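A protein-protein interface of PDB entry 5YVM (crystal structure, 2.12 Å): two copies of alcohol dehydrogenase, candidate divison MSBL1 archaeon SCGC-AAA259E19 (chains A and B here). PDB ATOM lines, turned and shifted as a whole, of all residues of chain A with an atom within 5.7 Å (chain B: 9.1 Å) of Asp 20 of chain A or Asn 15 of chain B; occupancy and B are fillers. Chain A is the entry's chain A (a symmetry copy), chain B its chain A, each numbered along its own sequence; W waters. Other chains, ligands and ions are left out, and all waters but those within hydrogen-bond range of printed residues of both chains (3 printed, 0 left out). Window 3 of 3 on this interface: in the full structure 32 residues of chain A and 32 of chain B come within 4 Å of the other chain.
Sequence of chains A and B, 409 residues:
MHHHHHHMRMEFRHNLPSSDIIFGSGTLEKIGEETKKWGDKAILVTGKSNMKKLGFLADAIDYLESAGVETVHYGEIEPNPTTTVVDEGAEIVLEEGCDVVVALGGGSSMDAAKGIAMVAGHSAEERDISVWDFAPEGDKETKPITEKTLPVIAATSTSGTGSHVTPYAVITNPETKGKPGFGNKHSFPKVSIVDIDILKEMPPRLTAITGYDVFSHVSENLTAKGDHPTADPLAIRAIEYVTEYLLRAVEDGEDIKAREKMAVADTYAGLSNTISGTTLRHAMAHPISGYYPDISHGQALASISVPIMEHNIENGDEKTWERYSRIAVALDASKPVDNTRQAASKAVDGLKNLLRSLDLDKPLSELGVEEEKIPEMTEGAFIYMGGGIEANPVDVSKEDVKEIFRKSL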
ATOM      1  N   SER A  18      -1.184  -9.874  20.451  1.00  0.00           N
ATOM      2  CA  SER A  18      -0.485 -11.108  20.093  1.00  0.00           C
ATOM      3  C   SER A  18       0.640 -10.841  19.090  1.00  0.00           C
ATOM      4  O   SER A  18       0.473 -10.074  18.140  1.00  0.00           O
ATOM      5  CB  SER A  18      -1.499 -12.114  19.520  1.00  0.00           C
ATOM      6  OG  SER A  18      -0.880 -13.019  18.610  1.00  0.00           O
ATOM      7  N   SER A  19       1.810 -11.431  19.338  1.00  0.00           N
ATOM      8  CA  SER A  19       2.954 -11.267  18.453  1.00  0.00           C
ATOM      9  C   SER A  19       3.511 -12.639  18.091  1.00  0.00           C
ATOM     10  O   SER A  19       3.475 -13.577  18.899  1.00  0.00           O
ATOM     11  CB  SER A  19       4.043 -10.382  19.086  1.00  0.00           C
ATOM     12  OG  SER A  19       4.361 -10.790  20.416  1.00  0.00           O
ATOM     13  N   ASP A  20       4.020 -12.734  16.861  1.00  0.00           N
ATOM     14  CA  ASP A  20       4.518 -13.967  16.247  1.00  0.00           C
ATOM     15  C   ASP A  20       5.691 -13.500  15.395  1.00  0.00           C
ATOM     16  O   ASP A  20       5.481 -12.850  14.370  1.00  0.00           O
ATOM     17  CB  ASP A  20       3.436 -14.631  15.399  1.00  0.00           C
ATOM     18  CG  ASP A  20       3.885 -15.932  14.739  1.00  0.00           C
ATOM     19  OD1 ASP A  20       5.074 -16.327  14.825  1.00  0.00           O
ATOM     20  OD2 ASP A  20       3.023 -16.576  14.103  1.00  0.00           O
ATOM     21  N   ILE A  21       6.917 -13.750  15.851  1.00  0.00           N
ATOM     22  CA  ILE A  21       8.105 -13.165  15.238  1.00  0.00           C
ATOM     23  C   ILE A  21       8.971 -14.295  14.735  1.00  0.00           C
ATOM     24  O   ILE A  21       9.339 -15.194  15.496  1.00  0.00           O
ATOM     25  CB  ILE A  21       8.883 -12.276  16.212  1.00  0.00           C
ATOM     26  CG1 ILE A  21       7.965 -11.186  16.753  1.00  0.00           C
ATOM     27  CG2 ILE A  21      10.106 -11.686  15.524  1.00  0.00           C
ATOM     28  CD1 ILE A  21       8.535 -10.429  17.936  1.00  0.00           C
ATOM     29  N   ILE A  22       9.293 -14.247  13.459  1.00  0.00           N
ATOM     30  CA  ILE A  22      10.154 -15.214  12.806  1.00  0.00           C
ATOM     31  C   ILE A  22      11.443 -14.480  12.516  1.00  0.00           C
ATOM     32  O   ILE A  22      11.487 -13.608  11.644  1.00  0.00           O
ATOM     33  CB  ILE A  22       9.514 -15.755  11.525  1.00  0.00           C
ATOM     34  CG1 ILE A  22       8.182 -16.438  11.866  1.00  0.00           C
ATOM     35  CG2 ILE A  22      10.472 -16.674  10.799  1.00  0.00           C
ATOM     36  CD1 ILE A  22       7.347 -16.749  10.612  1.00  0.00           C
ATOM     37  N   GLU A  34       3.084 -18.431   5.775  1.00  0.00           N
ATOM     38  CA  GLU A  34       2.415 -17.674   6.827  1.00  0.00           C
ATOM     39  C   GLU A  34       1.309 -16.793   6.263  1.00  0.00           C
ATOM     40  O   GLU A  34       0.239 -16.675   6.872  1.00  0.00           O
ATOM     41  CB  GLU A  34       3.429 -16.837   7.613  1.00  0.00           C
ATOM     42  CG  GLU A  34       4.611 -17.651   8.151  1.00  0.00           C
ATOM     43  CD  GLU A  34       4.240 -18.546   9.319  1.00  0.00           C
ATOM     44  OE1 GLU A  34       4.933 -19.572   9.522  1.00  0.00           O
ATOM     45  OE2 GLU A  34       3.256 -18.247  10.042  1.00  0.00           O
ATOM     46  N   LYS A  37      -1.952 -18.753   5.649  1.00  0.00           N
ATOM     47  CA  LYS A  37      -2.781 -18.958   6.824  1.00  0.00           C
ATOM     48  C   LYS A  37      -3.812 -17.853   6.970  1.00  0.00           C
ATOM     49  O   LYS A  37      -4.856 -18.069   7.591  1.00  0.00           O
ATOM     50  CB  LYS A  37      -1.904 -19.018   8.088  1.00  0.00           C
ATOM     51  CG  LYS A  37      -0.942 -20.197   8.162  1.00  0.00           C
ATOM     52  CD  LYS A  37       0.043 -19.995   9.345  1.00  0.00           C
ATOM     53  CE  LYS A  37       0.832 -21.269   9.704  1.00  0.00           C
ATOM     54  NZ  LYS A  37       1.902 -20.972  10.741  1.00  0.00           N
ATOM     55  N   PHE A 188      -2.150  -4.658  14.319  1.00  0.00           N
ATOM     56  CA  PHE A 188      -0.847  -5.196  14.674  1.00  0.00           C
ATOM     57  C   PHE A 188      -0.604  -6.419  13.798  1.00  0.00           C
ATOM     58  O   PHE A 188      -1.533  -7.211  13.591  1.00  0.00           O
ATOM     59  CB  PHE A 188      -0.842  -5.532  16.185  1.00  0.00           C
ATOM     60  CG  PHE A 188       0.515  -5.845  16.766  1.00  0.00           C
ATOM     61  CD1 PHE A 188       1.159  -7.028  16.428  1.00  0.00           C
ATOM     62  CD2 PHE A 188       1.112  -5.000  17.709  1.00  0.00           C
ATOM     63  CE1 PHE A 188       2.409  -7.365  16.976  1.00  0.00           C
ATOM     64  CE2 PHE A 188       2.370  -5.308  18.254  1.00  0.00           C
ATOM     65  CZ  PHE A 188       3.012  -6.512  17.882  1.00  0.00           C
ATOM     66  N   PRO A 189       0.581  -6.572  13.198  1.00  0.00           N
ATOM     67  CA  PRO A 189       0.791  -7.658  12.227  1.00  0.00           C
ATOM     68  C   PRO A 189       0.588  -9.046  12.814  1.00  0.00           C
ATOM     69  O   PRO A 189       1.011  -9.340  13.936  1.00  0.00           O
ATOM     70  CB  PRO A 189       2.244  -7.448  11.776  1.00  0.00           C
ATOM     71  CG  PRO A 189       2.416  -5.982  11.903  1.00  0.00           C
ATOM     72  CD  PRO A 189       1.720  -5.638  13.206  1.00  0.00           C
ATOM     73  N   LYS A 190      -0.086  -9.901  12.039  1.00  0.00           N
ATOM     74  CA  LYS A 190      -0.366 -11.259  12.495  1.00  0.00           C
ATOM     75  C   LYS A 190       0.919 -12.064  12.567  1.00  0.00           C
ATOM     76  O   LYS A 190       1.080 -12.922  13.451  1.00  0.00           O
ATOM     77  CB  LYS A 190      -1.376 -11.948  11.575  1.00  0.00           C
ATOM     78  CG  LYS A 190      -2.644 -11.149  11.337  1.00  0.00           C
ATOM     79  CD  LYS A 190      -3.418 -10.885  12.639  1.00  0.00           C
ATOM     80  CE  LYS A 190      -4.811 -10.358  12.316  1.00  0.00           C
ATOM     81  NZ  LYS A 190      -5.387  -9.544  13.422  1.00  0.00           N
ATOM     82  N   VAL A 191       1.849 -11.784  11.655  1.00  0.00           N
ATOM     83  CA  VAL A 191       3.148 -12.436  11.614  1.00  0.00           C
ATOM     84  C   VAL A 191       4.173 -11.392  11.217  1.00  0.00           C
ATOM     85  O   VAL A 191       3.926 -10.575  10.326  1.00  0.00           O
ATOM     86  CB  VAL A 191       3.206 -13.615  10.624  1.00  0.00           C
ATOM     87  CG1 VAL A 191       4.509 -14.400  10.844  1.00  0.00           C
ATOM     88  CG2 VAL A 191       1.975 -14.504  10.717  1.00  0.00           C
ATOM     89  N   SER A 192       5.324 -11.430  11.876  1.00  0.00           N
ATOM     90  CA  SER A 192       6.400 -10.468  11.687  1.00  0.00           C
ATOM     91  C   SER A 192       7.641 -11.258  11.300  1.00  0.00           C
ATOM     92  O   SER A 192       8.068 -12.145  12.048  1.00  0.00           O
ATOM     93  CB  SER A 192       6.643  -9.663  12.973  1.00  0.00           C
ATOM     94  OG  SER A 192       5.403  -9.185  13.497  1.00  0.00           O
ATOM     95  N   ILE A 193       8.208 -10.957  10.142  1.00  0.00           N
ATOM     96  CA  ILE A 193       9.397 -11.649   9.655  1.00  0.00           C
ATOM     97  C   ILE A 193      10.575 -10.681   9.669  1.00  0.00           C
ATOM     98  O   ILE A 193      10.507  -9.588   9.098  1.00  0.00           O
ATOM     99  CB  ILE A 193       9.169 -12.224   8.253  1.00  0.00           C
ATOM    100  CG1 ILE A 193       8.116 -13.352   8.326  1.00  0.00           C
ATOM    101  CG2 ILE A 193      10.476 -12.735   7.675  1.00  0.00           C
ATOM    102  CD1 ILE A 193       7.425 -13.609   6.966  1.00  0.00           C
ATOM    103  N   PHE B  12      15.247 -17.686  15.765  1.00  0.00           N
ATOM    104  CA  PHE B  12      14.226 -18.024  16.746  1.00  0.00           C
ATOM    105  C   PHE B  12      12.850 -17.681  16.194  1.00  0.00           C
ATOM    106  O   PHE B  12      12.703 -16.921  15.234  1.00  0.00           O
ATOM    107  CB  PHE B  12      14.466 -17.316  18.093  1.00  0.00           C
ATOM    108  CG  PHE B  12      14.359 -15.811  18.031  1.00  0.00           C
ATOM    109  CD1 PHE B  12      15.462 -15.045  17.679  1.00  0.00           C
ATOM    110  CD2 PHE B  12      13.164 -15.166  18.348  1.00  0.00           C
ATOM    111  CE1 PHE B  12      15.376 -13.674  17.642  1.00  0.00           C
ATOM    112  CE2 PHE B  12      13.060 -13.792  18.298  1.00  0.00           C
ATOM    113  CZ  PHE B  12      14.166 -13.046  17.947  1.00  0.00           C
ATOM    114  N   ARG B  13      11.840 -18.283  16.811  1.00  0.00           N
ATOM    115  CA  ARG B  13      10.466 -17.864  16.614  1.00  0.00           C
ATOM    116  C   ARG B  13       9.917 -17.479  17.975  1.00  0.00           C
ATOM    117  O   ARG B  13       9.960 -18.272  18.926  1.00  0.00           O
ATOM    118  CB  ARG B  13       9.615 -18.950  15.939  1.00  0.00           C
ATOM    119  CG  ARG B  13       8.223 -18.441  15.493  1.00  0.00           C
ATOM    120  CD  ARG B  13       7.605 -19.323  14.431  1.00  0.00           C
ATOM    121  NE  ARG B  13       6.356 -18.753  13.943  1.00  0.00           N
ATOM    122  CZ  ARG B  13       5.742 -19.134  12.825  1.00  0.00           C
ATOM    123  NH1 ARG B  13       6.275 -20.082  12.060  1.00  0.00           N
ATOM    124  NH2 ARG B  13       4.601 -18.553  12.452  1.00  0.00           N
ATOM    125  N   HIS B  14       9.439 -16.247  18.070  1.00  0.00           N
ATOM    126  CA  HIS B  14       8.823 -15.707  19.270  1.00  0.00           C
ATOM    127  C   HIS B  14       7.306 -15.784  19.111  1.00  0.00           C
ATOM    128  O   HIS B  14       6.763 -15.322  18.109  1.00  0.00           O
ATOM    129  CB  HIS B  14       9.309 -14.276  19.450  1.00  0.00           C
ATOM    130  CG  HIS B  14       8.532 -13.463  20.430  1.00  0.00           C
ATOM    131  ND1 HIS B  14       8.981 -13.223  21.709  1.00  0.00           N
ATOM    132  CD2 HIS B  14       7.371 -12.777  20.301  1.00  0.00           C
ATOM    133  CE1 HIS B  14       8.110 -12.454  22.340  1.00  0.00           C
ATOM    134  NE2 HIS B  14       7.134 -12.157  21.502  1.00  0.00           N
ATOM    135  N   ASN B  15       6.633 -16.394  20.084  1.00  0.00           N
ATOM    136  CA  ASN B  15       5.183 -16.463  20.084  1.00  0.00           C
ATOM    137  C   ASN B  15       4.689 -16.033  21.450  1.00  0.00           C
ATOM    138  O   ASN B  15       5.033 -16.650  22.471  1.00  0.00           O
ATOM    139  CB  ASN B  15       4.692 -17.870  19.737  1.00  0.00           C
ATOM    140  CG  ASN B  15       4.951 -18.224  18.276  1.00  0.00           C
ATOM    141  OD1 ASN B  15       5.752 -19.117  17.973  1.00  0.00           O
ATOM    142  ND2 ASN B  15       4.273 -17.529  17.361  1.00  0.00           N
ATOM    143  N   LEU B  16       3.899 -14.981  21.468  1.00  0.00           N
ATOM    144  CA  LEU B  16       3.370 -14.464  22.717  1.00  0.00           C
ATOM    145  C   LEU B  16       1.937 -14.038  22.473  1.00  0.00           C
ATOM    146  O   LEU B  16       1.693 -13.144  21.646  1.00  0.00           O
ATOM    147  CB  LEU B  16       4.189 -13.284  23.221  1.00  0.00           C
ATOM    148  CG  LEU B  16       3.667 -12.644  24.487  1.00  0.00           C
ATOM    149  CD1 LEU B  16       3.710 -13.649  25.626  1.00  0.00           C
ATOM    150  CD2 LEU B  16       4.551 -11.415  24.795  1.00  0.00           C
ATOM    151  N   PRO B  17       0.970 -14.670  23.130  1.00  0.00           N
ATOM    152  CA  PRO B  17      -0.433 -14.297  22.908  1.00  0.00           C
ATOM    153  C   PRO B  17      -0.694 -12.913  23.470  1.00  0.00           C
ATOM    154  O   PRO B  17       0.046 -12.426  24.326  1.00  0.00           O
ATOM    155  CB  PRO B  17      -1.221 -15.372  23.683  1.00  0.00           C
ATOM    156  CG  PRO B  17      -0.270 -16.536  23.821  1.00  0.00           C
ATOM    157  CD  PRO B  17       1.098 -15.874  23.972  1.00  0.00           C
ATOM    158  N   SER B  18      -1.774 -12.296  22.984  1.00  0.00           N
ATOM    159  CA  SER B  18      -2.222 -10.990  23.470  1.00  0.00           C
ATOM    160  C   SER B  18      -2.307 -10.962  24.997  1.00  0.00           C
ATOM    161  O   SER B  18      -2.782 -11.911  25.623  1.00  0.00           O
ATOM    162  CB  SER B  18      -3.588 -10.661  22.841  1.00  0.00           C
ATOM    163  OG  SER B  18      -4.353  -9.797  23.677  1.00  0.00           O
ATOM    164  N   VAL B 165      -0.289 -14.614  33.224  1.00  0.00           N
ATOM    165  CA  VAL B 165       0.164 -14.279  31.884  1.00  0.00           C
ATOM    166  C   VAL B 165       0.941 -15.453  31.280  1.00  0.00           C
ATOM    167  O   VAL B 165       1.994 -15.267  30.672  1.00  0.00           O
ATOM    168  CB  VAL B 165       1.011 -12.991  31.899  1.00  0.00           C
ATOM    169  CG1 VAL B 165       0.127 -11.766  32.123  1.00  0.00           C
ATOM    170  CG2 VAL B 165       2.085 -13.064  32.997  1.00  0.00           C
ATOM    171  N   PRO B 167      -0.028 -19.321  28.978  1.00  0.00           N
ATOM    172  CA  PRO B 167      -1.067 -20.232  28.459  1.00  0.00           C
ATOM    173  C   PRO B 167      -1.248 -21.528  29.232  1.00  0.00           C
ATOM    174  O   PRO B 167      -2.180 -22.284  28.923  1.00  0.00           O
ATOM    175  CB  PRO B 167      -0.595 -20.529  27.031  1.00  0.00           C
ATOM    176  CG  PRO B 167       0.781 -19.979  26.860  1.00  0.00           C
ATOM    177  CD  PRO B 167       1.141 -19.187  28.079  1.00  0.00           C
ATOM    178  N   TYR B 168      -0.413 -21.819  30.215  1.00  0.00           N
ATOM    179  CA  TYR B 168      -0.245 -23.179  30.693  1.00  0.00           C
ATOM    180  C   TYR B 168      -1.142 -23.446  31.896  1.00  0.00           C
ATOM    181  O   TYR B 168      -1.414 -22.546  32.698  1.00  0.00           O
ATOM    182  CB  TYR B 168       1.229 -23.443  31.038  1.00  0.00           C
ATOM    183  CG  TYR B 168       2.168 -23.053  29.898  1.00  0.00           C
ATOM    184  CD1 TYR B 168       1.982 -23.548  28.602  1.00  0.00           C
ATOM    185  CD2 TYR B 168       3.212 -22.166  30.119  1.00  0.00           C
ATOM    186  CE1 TYR B 168       2.832 -23.173  27.554  1.00  0.00           C
ATOM    187  CE2 TYR B 168       4.066 -21.793  29.116  1.00  0.00           C
ATOM    188  CZ  TYR B 168       3.874 -22.282  27.826  1.00  0.00           C
ATOM    189  OH  TYR B 168       4.742 -21.878  26.839  1.00  0.00           O
ATOM    190  N   ASN B 184      -2.071 -23.260  25.256  1.00  0.00           N
ATOM    191  CA  ASN B 184      -1.554 -22.430  24.183  1.00  0.00           C
ATOM    192  C   ASN B 184      -2.283 -21.100  24.157  1.00  0.00           C
ATOM    193  O   ASN B 184      -2.887 -20.705  25.162  1.00  0.00           O
ATOM    194  CB  ASN B 184      -1.691 -23.165  22.856  1.00  0.00           C
ATOM    195  CG  ASN B 184      -3.148 -23.525  22.524  1.00  0.00           C
ATOM    196  OD1 ASN B 184      -4.097 -22.817  22.902  1.00  0.00           O
ATOM    197  ND2 ASN B 184      -3.321 -24.634  21.815  1.00  0.00           N
ATOM    198  N   LYS B 185      -2.303 -20.459  22.981  1.00  0.00           N
ATOM    199  CA  LYS B 185      -2.814 -19.096  22.854  1.00  0.00           C
ATOM    200  C   LYS B 185      -4.273 -19.002  23.289  1.00  0.00           C
ATOM    201  O   LYS B 185      -4.706 -17.962  23.803  1.00  0.00           O
ATOM    202  CB  LYS B 185      -2.677 -18.607  21.402  1.00  0.00           C
ATOM    203  CG  LYS B 185      -1.715 -19.375  20.498  1.00  0.00           C
ATOM    204  CD  LYS B 185      -0.407 -19.843  21.150  1.00  0.00           C
ATOM    205  CE  LYS B 185       0.225 -20.945  20.483  1.00  0.00           C
ATOM    206  NZ  LYS B 185       1.364 -21.507  21.278  1.00  0.00           N
ATOM    207  N   PHE B 188      -4.672 -18.609  27.166  1.00  0.00           N
ATOM    208  CA  PHE B 188      -3.983 -17.506  27.816  1.00  0.00           C
ATOM    209  C   PHE B 188      -5.045 -16.515  28.279  1.00  0.00           C
ATOM    210  O   PHE B 188      -6.001 -16.258  27.535  1.00  0.00           O
ATOM    211  CB  PHE B 188      -2.981 -16.883  26.813  1.00  0.00           C
ATOM    212  CG  PHE B 188      -2.000 -15.907  27.413  1.00  0.00           C
ATOM    213  CD1 PHE B 188      -2.439 -14.665  27.855  1.00  0.00           C
ATOM    214  CD2 PHE B 188      -0.631 -16.192  27.462  1.00  0.00           C
ATOM    215  CE1 PHE B 188      -1.546 -13.719  28.388  1.00  0.00           C
ATOM    216  CE2 PHE B 188       0.276 -15.270  28.010  1.00  0.00           C
ATOM    217  CZ  PHE B 188      -0.198 -14.018  28.466  1.00  0.00           C
ATOM    218  N   HIS B 228      16.483 -16.909  22.536  1.00  0.00           N
ATOM    219  CA  HIS B 228      15.174 -16.394  22.930  1.00  0.00           C
ATOM    220  C   HIS B 228      15.334 -14.970  23.448  1.00  0.00           C
ATOM    221  O   HIS B 228      15.004 -14.673  24.599  1.00  0.00           O
ATOM    222  CB  HIS B 228      14.530 -17.311  23.981  1.00  0.00           C
ATOM    223  CG  HIS B 228      15.525 -18.101  24.785  1.00  0.00           C
ATOM    224  ND1 HIS B 228      16.291 -17.537  25.784  1.00  0.00           N
ATOM    225  CD2 HIS B 228      15.893 -19.403  24.724  1.00  0.00           C
ATOM    226  CE1 HIS B 228      17.083 -18.459  26.308  1.00  0.00           C
ATOM    227  NE2 HIS B 228      16.853 -19.603  25.690  1.00  0.00           N
ATOM    228  N   THR B 230      13.783 -12.169  23.236  1.00  0.00           N
ATOM    229  CA  THR B 230      12.702 -11.314  23.712  1.00  0.00           C
ATOM    230  C   THR B 230      12.357 -11.622  25.162  1.00  0.00           C
ATOM    231  O   THR B 230      11.882 -10.730  25.882  1.00  0.00           O
ATOM    232  CB  THR B 230      11.476 -11.429  22.764  1.00  0.00           C
ATOM    233  OG1 THR B 230      11.074 -12.786  22.623  1.00  0.00           O
ATOM    234  CG2 THR B 230      11.836 -10.961  21.358  1.00  0.00           C
ATOM    235  N   ALA B 231      12.615 -12.856  25.622  1.00  0.00           N
ATOM    236  CA  ALA B 231      12.397 -13.209  27.019  1.00  0.00           C
ATOM    237  C   ALA B 231      13.510 -12.676  27.919  1.00  0.00           C
ATOM    238  O   ALA B 231      13.250 -12.332  29.079  1.00  0.00           O
ATOM    239  CB  ALA B 231      12.313 -14.735  27.172  1.00  0.00           C
ATOM    240  N   GLY B 270       6.043 -14.842  33.857  1.00  0.00           N
ATOM    241  CA  GLY B 270       5.024 -15.442  33.017  1.00  0.00           C
ATOM    242  C   GLY B 270       5.242 -15.123  31.551  1.00  0.00           C
ATOM    243  O   GLY B 270       5.193 -16.009  30.694  1.00  0.00           O
ATOM    244  N   LEU B 271       5.481 -13.850  31.240  1.00  0.00           N
ATOM    245  CA  LEU B 271       5.766 -13.458  29.866  1.00  0.00           C
ATOM    246  C   LEU B 271       6.983 -14.206  29.335  1.00  0.00           C
ATOM    247  O   LEU B 271       6.980 -14.728  28.201  1.00  0.00           O
ATOM    248  CB  LEU B 271       5.991 -11.944  29.805  1.00  0.00           C
ATOM    249  CG  LEU B 271       4.762 -11.105  30.197  1.00  0.00           C
ATOM    250  CD1 LEU B 271       5.071  -9.600  30.185  1.00  0.00           C
ATOM    251  CD2 LEU B 271       3.572 -11.409  29.278  1.00  0.00           C
ATOM    252  N   SER B 272       8.032 -14.268  30.167  1.00  0.00           N
ATOM    253  CA  SER B 272       9.265 -14.950  29.802  1.00  0.00           C
ATOM    254  C   SER B 272       9.054 -16.456  29.661  1.00  0.00           C
ATOM    255  O   SER B 272       9.596 -17.077  28.740  1.00  0.00           O
ATOM    256  CB  SER B 272      10.342 -14.632  30.853  1.00  0.00           C
ATOM    257  OG  SER B 272      11.433 -15.512  30.714  1.00  0.00           O
ATOM    258  N   ASN B 273       8.258 -17.062  30.546  1.00  0.00           N
ATOM    259  CA  ASN B 273       8.023 -18.505  30.441  1.00  0.00           C
ATOM    260  C   ASN B 273       7.131 -18.846  29.242  1.00  0.00           C
ATOM    261  O   ASN B 273       7.187 -19.962  28.711  1.00  0.00           O
ATOM    262  CB  ASN B 273       7.400 -19.020  31.735  1.00  0.00           C
ATOM    263  CG  ASN B 273       7.531 -20.524  31.887  1.00  0.00           C
ATOM    264  OD1 ASN B 273       8.439 -21.120  31.313  1.00  0.00           O
ATOM    265  ND2 ASN B 273       6.588 -21.157  32.614  1.00  0.00           N
ATOM    266  N   THR B 274       6.272 -17.931  28.823  1.00  0.00           N
ATOM    267  CA  THR B 274       5.537 -18.152  27.580  1.00  0.00           C
ATOM    268  C   THR B 274       6.475 -18.153  26.386  1.00  0.00           C
ATOM    269  O   THR B 274       6.422 -19.059  25.543  1.00  0.00           O
ATOM    270  CB  THR B 274       4.466 -17.078  27.392  1.00  0.00           C
ATOM    271  OG1 THR B 274       3.605 -17.069  28.534  1.00  0.00           O
ATOM    272  CG2 THR B 274       3.649 -17.371  26.140  1.00  0.00           C
ATOM    273  N   ILE B 275       7.327 -17.128  26.277  1.00  0.00           N
ATOM    274  CA  ILE B 275       8.210 -16.996  25.115  1.00  0.00           C
ATOM    275  C   ILE B 275       9.233 -18.121  25.084  1.00  0.00           C
ATOM    276  O   ILE B 275       9.458 -18.761  24.049  1.00  0.00           O
ATOM    277  CB  ILE B 275       8.928 -15.634  25.126  1.00  0.00           C
ATOM    278  CG1 ILE B 275       7.957 -14.471  24.915  1.00  0.00           C
ATOM    279  CG2 ILE B 275      10.014 -15.620  24.062  1.00  0.00           C
ATOM    280  CD1 ILE B 275       8.479 -13.191  25.486  1.00  0.00           C
ATOM    281  N   SER B 276       9.955 -18.298  26.194  1.00  0.00           N
ATOM    282  CA  SER B 276      10.992 -19.303  26.285  1.00  0.00           C
ATOM    283  C   SER B 276      10.344 -20.567  26.821  1.00  0.00           C
ATOM    284  O   SER B 276       9.199 -20.876  26.482  1.00  0.00           O
ATOM    285  CB  SER B 276      12.129 -18.828  27.198  1.00  0.00           C
ATOM    286  OG  SER B 276      13.209 -19.741  27.190  1.00  0.00           O
HETATM  287  O   HOH W   1       2.535 -19.435  14.421  1.00  0.00           O
HETATM  288  O   HOH W   2       2.160 -15.785  18.396  1.00  0.00           O
HETATM  289  O   HOH W   3       2.612 -10.226  22.219  1.00  0.00           O
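The side-chain carboxylate of Asp 20 of chain A lies within salt-bridge range of the guanidinium group of Arg 13 of chain B.
The side-chain carboxylate (OE2) of Glu 34 of chain A is in salt-bridge range of the guanidinium group (NH2) of Arg 13 of chain B (2.8 Å).
OG of Ser 19 of chain A is in hydrogen-bond range of NE2 of His 14 of chain B (3.3 Å).
The backbone carbonyl oxygen (O) of His 14 of chain B lies within hydrogen-bond range of the backbone NH (N) of Ile 21 of chain A, 2.8 Å away.
The side-chain amide nitrogen (ND2) of Asn 15 of chain B is in hydrogen-bond range of the side-chain carboxylate (OD1) of Asp 20 of chain A (2.9 Å).
N of Ser 19 of chain A sits at hydrogen-bond distance from O of Leu 16 of chain B (2.9 Å).
The backbone carbonyl oxygen of Asp 20 of chain A lies within hydrogen-bond range of the backbone NH of Ser 192 of chain A (2.9 Å).
The backbone NH of Ile 22 of chain A is in hydrogen-bond range of the backbone carbonyl oxygen of Ser 192 of chain A (2.8 Å).
NZ of Lys 37 of chain A is in salt-bridge range of OE2 of Glu 34 of chain A.
Among the printed residues, merely in contact across the chains: Ile 21 of chain A with Arg 13 of chain B (3.1 Å), Asp 20 of chain A with His 14 of chain B (3.2 Å), Ser 18 of chain A with Leu 16 of chain B (3.4 Å), Ser 18 of chain A with Ser 18 of chain B (3.4 Å), Ser 19 of chain A with Asn 15 of chain B (3.6 Å), Ile 22 of chain A with Arg 13 of chain B (3.6 Å), Ile 21 of chain A with Phe 12 of chain B (3.8 Å), Ser 18 of chain A with Pro 17 of chain B (3.8 Å) and Ile 22 of chain A with Phe 12 of chain B (3.9 Å).
Of the printed residues of chain B, Ser 18 of chain A touches Leu 16 (3.4 Å), Pro 17 (3.8 Å) and Ser 18 (3.4 Å).
Ser 19 of chain A touches just these residues of chain B: His 14, Asn 15 and Leu 16.
Of chain B, only Phe 12 (3.8 Å), Arg 13 (3.1 Å) and His 14 (2.8 Å) come within 4 Å of Ile 21 of chain A.
Of the printed residues of chain B, Glu 34 of chain A touches Arg 13 (2.8 Å).
Val 191 of chain A touches none of the printed residues of chain B.
Ser 192 of chain A touches none of the printed residues of chain B.
Of the printed residues of chain A, Arg 13 of chain B touches Asp 20 (2.9 Å), Ile 21 (3.1 Å), Ile 22 (3.6 Å) and Glu 34 (2.8 Å).
Of the printed residues of chain A, His 14 of chain B touches Ser 19 (3.3 Å), Asp 20 (3.2 Å) and Ile 21 (2.8 Å).
Printed residues of chain A within 4 Å of Pro 17 of chain B: Ser 18 (3.8 Å).
Printed residues of chain B that touch a printed residue of chain A: Phe 12, Arg 13, His 14, Asn 15, Leu 16, Pro 17 and Ser 18.
Of the 13 printed residues of chain A, 6 touch a printed residue of chain B.
Hydrophobic or aromatic side chains of chain A that line the printed part of chain B: Ile 21 and Ile 22.
Ser 18 of chain B touches its own counterpart, Ser 18 of chain A.
Positions printed for both chains: 18 and 188.
Water W3 lies within hydrogen-bond range of OG of Ser 19 of chain A and O of Leu 16 of chain B.
Water W2 bridges the backbone carbonyl oxygen of Ser 19 of chain A and the side-chain amide nitrogen of Asn 15 of chain B.
Water W1 lies within hydrogen-bond range of the side-chain carboxylate (OD2) of Asp 20 of chain A (2.9 Å) and the guanidinium group (NH2) of Arg 13 of chain B (3.0 Å).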
